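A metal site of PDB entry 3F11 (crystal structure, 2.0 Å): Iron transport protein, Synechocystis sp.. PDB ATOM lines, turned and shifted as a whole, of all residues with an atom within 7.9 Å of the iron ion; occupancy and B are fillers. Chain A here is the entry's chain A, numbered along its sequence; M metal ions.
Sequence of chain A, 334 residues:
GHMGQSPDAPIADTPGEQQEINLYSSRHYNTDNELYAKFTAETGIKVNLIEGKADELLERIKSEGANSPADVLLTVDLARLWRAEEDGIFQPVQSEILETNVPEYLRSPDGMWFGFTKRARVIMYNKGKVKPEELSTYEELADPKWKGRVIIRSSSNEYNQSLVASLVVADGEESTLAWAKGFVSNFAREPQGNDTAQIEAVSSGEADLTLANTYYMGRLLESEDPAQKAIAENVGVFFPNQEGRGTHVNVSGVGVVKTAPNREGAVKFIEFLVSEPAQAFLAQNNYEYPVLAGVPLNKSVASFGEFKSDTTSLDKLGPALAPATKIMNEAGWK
Five residues have an atom within 4 Å of the iron ion: His 28, Tyr 29, Tyr 159, Tyr 215 and Tyr 216.
The nearest printed residue that does not touch the iron ion is Arg 119 (4.1 Å).
The backbone NH (N) of Tyr 159 is in hydrogen-bond range of the side-chain amide oxygen (OD1) of Asn 157, 2.9 Å away.
The side-chain hydroxyl (OH) of Tyr 215 lies close to the side-chain amide nitrogen (ND2) of Asn 213 (3.0 Å).
The guanidinium group (NH1) of Arg 119 sits close to the side-chain hydroxyl (OH) of Tyr 159 (3.5 Å).
The guanidinium group (NH2) of Arg 119 sits close to the side-chain hydroxyl (OH) of Tyr 29 (2.8 Å).
The side-chain hydroxyl (OH) of Tyr 215 sits close to the guanidinium group (NH1) of Arg 119 (3.0 Å).
The iron ion is bound by the side-chain hydroxyl of Tyr 159, the side-chain hydroxyl of Tyr 29, the side-chain hydroxyl of Tyr 215, the side-chain hydroxyl of Tyr 216 and a ring nitrogen (NE2) of His 28.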
ATOM      1  N   SER A  26      -1.727 -26.349   8.829  1.00  0.00           N
ATOM      2  CA  SER A  26      -0.980 -25.198   9.268  1.00  0.00           C
ATOM      3  C   SER A  26       0.002 -25.610  10.372  1.00  0.00           C
ATOM      4  O   SER A  26       0.673 -24.760  10.964  1.00  0.00           O
ATOM      5  CB  SER A  26      -1.918 -24.069   9.747  1.00  0.00           C
ATOM      6  OG  SER A  26      -2.877 -24.506  10.696  1.00  0.00           O
ATOM      7  N   ARG A  27       0.079 -26.909  10.659  1.00  0.00           N
ATOM      8  CA  ARG A  27       1.066 -27.385  11.634  1.00  0.00           C
ATOM      9  C   ARG A  27       2.366 -27.191  10.871  1.00  0.00           C
ATOM     10  O   ARG A  27       2.426 -27.430   9.666  1.00  0.00           O
ATOM     11  CB  ARG A  27       0.876 -28.864  11.985  1.00  0.00           C
ATOM     12  CG  ARG A  27      -0.165 -29.115  13.066  1.00  0.00           C
ATOM     13  CD  ARG A  27      -0.249 -30.602  13.415  1.00  0.00           C
ATOM     14  NE  ARG A  27       0.858 -31.068  14.252  1.00  0.00           N
ATOM     15  CZ  ARG A  27       0.966 -30.848  15.558  1.00  0.00           C
ATOM     16  NH1 ARG A  27       0.030 -30.147  16.194  1.00  0.00           N
ATOM     17  NH2 ARG A  27       1.980 -31.348  16.233  1.00  0.00           N
ATOM     18  N   HIS A  28       3.406 -26.783  11.584  1.00  0.00           N
ATOM     19  CA  HIS A  28       4.702 -26.471  10.988  1.00  0.00           C
ATOM     20  C   HIS A  28       5.875 -27.109  11.734  1.00  0.00           C
ATOM     21  O   HIS A  28       6.892 -26.432  11.955  1.00  0.00           O
ATOM     22  CB  HIS A  28       4.879 -24.957  11.014  1.00  0.00           C
ATOM     23  CG  HIS A  28       4.814 -24.379  12.403  1.00  0.00           C
ATOM     24  ND1 HIS A  28       5.940 -24.028  13.107  1.00  0.00           N
ATOM     25  CD2 HIS A  28       3.763 -24.143  13.215  1.00  0.00           C
ATOM     26  CE1 HIS A  28       5.589 -23.592  14.307  1.00  0.00           C
ATOM     27  NE2 HIS A  28       4.266 -23.662  14.399  1.00  0.00           N
ATOM     28  N   TYR A  29       5.756 -28.372  12.114  1.00  0.00           N
ATOM     29  CA  TYR A  29       6.806 -29.031  12.876  1.00  0.00           C
ATOM     30  C   TYR A  29       7.581 -30.111  12.119  1.00  0.00           C
ATOM     31  O   TYR A  29       7.034 -30.776  11.239  1.00  0.00           O
ATOM     32  CB  TYR A  29       6.201 -29.620  14.152  1.00  0.00           C
ATOM     33  CG  TYR A  29       5.330 -28.605  14.870  1.00  0.00           C
ATOM     34  CD1 TYR A  29       3.932 -28.678  14.805  1.00  0.00           C
ATOM     35  CD2 TYR A  29       5.912 -27.539  15.553  1.00  0.00           C
ATOM     36  CE1 TYR A  29       3.134 -27.702  15.406  1.00  0.00           C
ATOM     37  CE2 TYR A  29       5.122 -26.559  16.158  1.00  0.00           C
ATOM     38  CZ  TYR A  29       3.736 -26.637  16.075  1.00  0.00           C
ATOM     39  OH  TYR A  29       2.973 -25.657  16.654  1.00  0.00           O
ATOM     40  N   VAL A  76      -3.479 -25.015  14.175  1.00  0.00           N
ATOM     41  CA  VAL A  76      -2.767 -24.975  15.448  1.00  0.00           C
ATOM     42  C   VAL A  76      -3.397 -23.828  16.220  1.00  0.00           C
ATOM     43  O   VAL A  76      -2.725 -23.111  16.960  1.00  0.00           O
ATOM     44  CB  VAL A  76      -1.254 -24.706  15.277  1.00  0.00           C
ATOM     45  CG1 VAL A  76      -0.588 -25.914  14.614  1.00  0.00           C
ATOM     46  CG2 VAL A  76      -1.023 -23.444  14.444  1.00  0.00           C
ATOM     47  N   ARG A 119      -1.804 -26.727  23.977  1.00  0.00           N
ATOM     48  CA  ARG A 119      -0.573 -25.998  24.216  1.00  0.00           C
ATOM     49  C   ARG A 119      -0.931 -24.743  25.008  1.00  0.00           C
ATOM     50  O   ARG A 119      -1.987 -24.145  24.795  1.00  0.00           O
ATOM     51  CB  ARG A 119       0.118 -25.620  22.896  1.00  0.00           C
ATOM     52  CG  ARG A 119      -0.759 -24.909  21.861  1.00  0.00           C
ATOM     53  CD  ARG A 119      -1.469 -25.877  20.906  1.00  0.00           C
ATOM     54  NE  ARG A 119      -0.543 -26.581  20.017  1.00  0.00           N
ATOM     55  CZ  ARG A 119       0.167 -26.002  19.040  1.00  0.00           C
ATOM     56  NH1 ARG A 119       0.067 -24.694  18.830  1.00  0.00           N
ATOM     57  NH2 ARG A 119       0.962 -26.730  18.274  1.00  0.00           N
ATOM     58  N   ARG A 121       0.023 -20.844  26.263  1.00  0.00           N
ATOM     59  CA  ARG A 121       0.838 -19.687  25.910  1.00  0.00           C
ATOM     60  C   ARG A 121       1.168 -19.086  27.270  1.00  0.00           C
ATOM     61  O   ARG A 121       0.305 -18.498  27.927  1.00  0.00           O
ATOM     62  CB  ARG A 121       0.065 -18.684  25.046  1.00  0.00           C
ATOM     63  CG  ARG A 121       0.979 -17.723  24.291  1.00  0.00           C
ATOM     64  CD  ARG A 121       0.280 -17.091  23.078  1.00  0.00           C
ATOM     65  NE  ARG A 121       1.207 -16.332  22.241  1.00  0.00           N
ATOM     66  CZ  ARG A 121       2.232 -16.870  21.584  1.00  0.00           C
ATOM     67  NH1 ARG A 121       2.466 -18.170  21.656  1.00  0.00           N
ATOM     68  NH2 ARG A 121       3.016 -16.106  20.842  1.00  0.00           N
ATOM     69  N   ARG A 153       6.278 -11.912  19.500  1.00  0.00           N
ATOM     70  CA  ARG A 153       6.182 -11.954  18.048  1.00  0.00           C
ATOM     71  C   ARG A 153       5.035 -11.062  17.558  1.00  0.00           C
ATOM     72  O   ARG A 153       4.234 -10.574  18.358  1.00  0.00           O
ATOM     73  CB  ARG A 153       5.975 -13.399  17.574  1.00  0.00           C
ATOM     74  CG  ARG A 153       4.600 -13.963  17.872  1.00  0.00           C
ATOM     75  CD  ARG A 153       4.573 -15.448  17.590  1.00  0.00           C
ATOM     76  NE  ARG A 153       4.896 -15.777  16.201  1.00  0.00           N
ATOM     77  CZ  ARG A 153       5.088 -17.022  15.771  1.00  0.00           C
ATOM     78  NH1 ARG A 153       4.988 -18.033  16.627  1.00  0.00           N
ATOM     79  NH2 ARG A 153       5.364 -17.267  14.500  1.00  0.00           N
ATOM     80  N   ASN A 157       0.366 -13.096  14.121  1.00  0.00           N
ATOM     81  CA  ASN A 157       0.341 -14.490  14.548  1.00  0.00           C
ATOM     82  C   ASN A 157      -0.939 -14.866  15.290  1.00  0.00           C
ATOM     83  O   ASN A 157      -1.391 -14.147  16.174  1.00  0.00           O
ATOM     84  CB  ASN A 157       1.570 -14.788  15.413  1.00  0.00           C
ATOM     85  CG  ASN A 157       1.503 -16.141  16.083  1.00  0.00           C
ATOM     86  OD1 ASN A 157       1.141 -16.253  17.258  1.00  0.00           O
ATOM     87  ND2 ASN A 157       1.848 -17.191  15.349  1.00  0.00           N
ATOM     88  N   TYR A 159      -1.528 -17.260  17.474  1.00  0.00           N
ATOM     89  CA  TYR A 159      -1.380 -17.601  18.883  1.00  0.00           C
ATOM     90  C   TYR A 159      -1.649 -16.312  19.683  1.00  0.00           C
ATOM     91  O   TYR A 159      -2.333 -16.341  20.700  1.00  0.00           O
ATOM     92  CB  TYR A 159       0.045 -18.083  19.181  1.00  0.00           C
ATOM     93  CG  TYR A 159       0.486 -19.316  18.401  1.00  0.00           C
ATOM     94  CD1 TYR A 159       1.833 -19.548  18.146  1.00  0.00           C
ATOM     95  CD2 TYR A 159      -0.436 -20.269  17.976  1.00  0.00           C
ATOM     96  CE1 TYR A 159       2.264 -20.690  17.480  1.00  0.00           C
ATOM     97  CE2 TYR A 159      -0.021 -21.426  17.309  1.00  0.00           C
ATOM     98  CZ  TYR A 159       1.330 -21.632  17.066  1.00  0.00           C
ATOM     99  OH  TYR A 159       1.755 -22.785  16.444  1.00  0.00           O
ATOM    100  N   ASP A 195       8.118 -17.655  18.100  1.00  0.00           N
ATOM    101  CA  ASP A 195       8.197 -17.881  19.546  1.00  0.00           C
ATOM    102  C   ASP A 195       9.595 -18.272  20.012  1.00  0.00           C
ATOM    103  O   ASP A 195      10.066 -17.789  21.046  1.00  0.00           O
ATOM    104  CB  ASP A 195       7.210 -18.969  19.984  1.00  0.00           C
ATOM    105  CG  ASP A 195       5.803 -18.447  20.207  1.00  0.00           C
ATOM    106  OD1 ASP A 195       4.988 -19.173  20.832  1.00  0.00           O
ATOM    107  OD2 ASP A 195       5.486 -17.328  19.752  1.00  0.00           O
ATOM    108  N   ASN A 213       4.460 -20.502  23.410  1.00  0.00           N
ATOM    109  CA  ASN A 213       3.806 -21.769  23.693  1.00  0.00           C
ATOM    110  C   ASN A 213       4.780 -22.718  24.369  1.00  0.00           C
ATOM    111  O   ASN A 213       5.960 -22.797  24.017  1.00  0.00           O
ATOM    112  CB  ASN A 213       3.250 -22.405  22.413  1.00  0.00           C
ATOM    113  CG  ASN A 213       2.084 -21.615  21.826  1.00  0.00           C
ATOM    114  OD1 ASN A 213       1.432 -20.842  22.517  1.00  0.00           O
ATOM    115  ND2 ASN A 213       1.819 -21.840  20.536  1.00  0.00           N
ATOM    116  N   TYR A 215       5.356 -25.969  24.327  1.00  0.00           N
ATOM    117  CA  TYR A 215       6.105 -26.954  23.549  1.00  0.00           C
ATOM    118  C   TYR A 215       7.375 -26.413  22.894  1.00  0.00           C
ATOM    119  O   TYR A 215       8.258 -27.182  22.535  1.00  0.00           O
ATOM    120  CB  TYR A 215       5.177 -27.625  22.522  1.00  0.00           C
ATOM    121  CG  TYR A 215       4.579 -26.683  21.512  1.00  0.00           C
ATOM    122  CD1 TYR A 215       5.286 -26.326  20.365  1.00  0.00           C
ATOM    123  CD2 TYR A 215       3.318 -26.124  21.709  1.00  0.00           C
ATOM    124  CE1 TYR A 215       4.761 -25.431  19.452  1.00  0.00           C
ATOM    125  CE2 TYR A 215       2.780 -25.217  20.807  1.00  0.00           C
ATOM    126  CZ  TYR A 215       3.509 -24.871  19.678  1.00  0.00           C
ATOM    127  OH  TYR A 215       3.011 -23.943  18.797  1.00  0.00           O
ATOM    128  N   TYR A 216       7.490 -25.091  22.762  1.00  0.00           N
ATOM    129  CA  TYR A 216       8.704 -24.517  22.177  1.00  0.00           C
ATOM    130  C   TYR A 216       9.853 -24.619  23.183  1.00  0.00           C
ATOM    131  O   TYR A 216      11.001 -24.825  22.805  1.00  0.00           O
ATOM    132  CB  TYR A 216       8.513 -23.042  21.790  1.00  0.00           C
ATOM    133  CG  TYR A 216       7.653 -22.852  20.563  1.00  0.00           C
ATOM    134  CD1 TYR A 216       6.423 -22.196  20.633  1.00  0.00           C
ATOM    135  CD2 TYR A 216       8.039 -23.394  19.333  1.00  0.00           C
ATOM    136  CE1 TYR A 216       5.596 -22.098  19.527  1.00  0.00           C
ATOM    137  CE2 TYR A 216       7.218 -23.295  18.215  1.00  0.00           C
ATOM    138  CZ  TYR A 216       5.997 -22.646  18.321  1.00  0.00           C
ATOM    139  OH  TYR A 216       5.159 -22.583  17.222  1.00  0.00           O
ATOM    140  N   ASN A 286       6.697 -33.991  20.153  1.00  0.00           N
ATOM    141  CA  ASN A 286       6.461 -32.602  19.793  1.00  0.00           C
ATOM    142  C   ASN A 286       6.206 -31.742  21.027  1.00  0.00           C
ATOM    143  O   ASN A 286       5.922 -30.556  20.928  1.00  0.00           O
ATOM    144  CB  ASN A 286       5.301 -32.439  18.817  1.00  0.00           C
ATOM    145  CG  ASN A 286       5.448 -31.167  17.990  1.00  0.00           C
ATOM    146  OD1 ASN A 286       4.487 -30.427  17.765  1.00  0.00           O
ATOM    147  ND2 ASN A 286       6.669 -30.907  17.534  1.00  0.00           N
ATOM    148  N   GLU A 288       3.766 -31.406  23.168  1.00  0.00           N
ATOM    149  CA  GLU A 288       2.456 -30.799  23.408  1.00  0.00           C
ATOM    150  C   GLU A 288       1.720 -31.594  24.481  1.00  0.00           C
ATOM    151  O   GLU A 288       2.183 -32.662  24.896  1.00  0.00           O
ATOM    152  CB  GLU A 288       1.629 -30.775  22.121  1.00  0.00           C
ATOM    153  CG  GLU A 288       2.241 -29.924  21.013  1.00  0.00           C
ATOM    154  CD  GLU A 288       1.594 -30.149  19.663  1.00  0.00           C
ATOM    155  OE1 GLU A 288       0.574 -29.502  19.362  1.00  0.00           O
ATOM    156  OE2 GLU A 288       2.111 -30.994  18.897  1.00  0.00           O
HETATM  157 FE    FE M   1       3.485 -23.696  16.831  1.00  0.00          FE
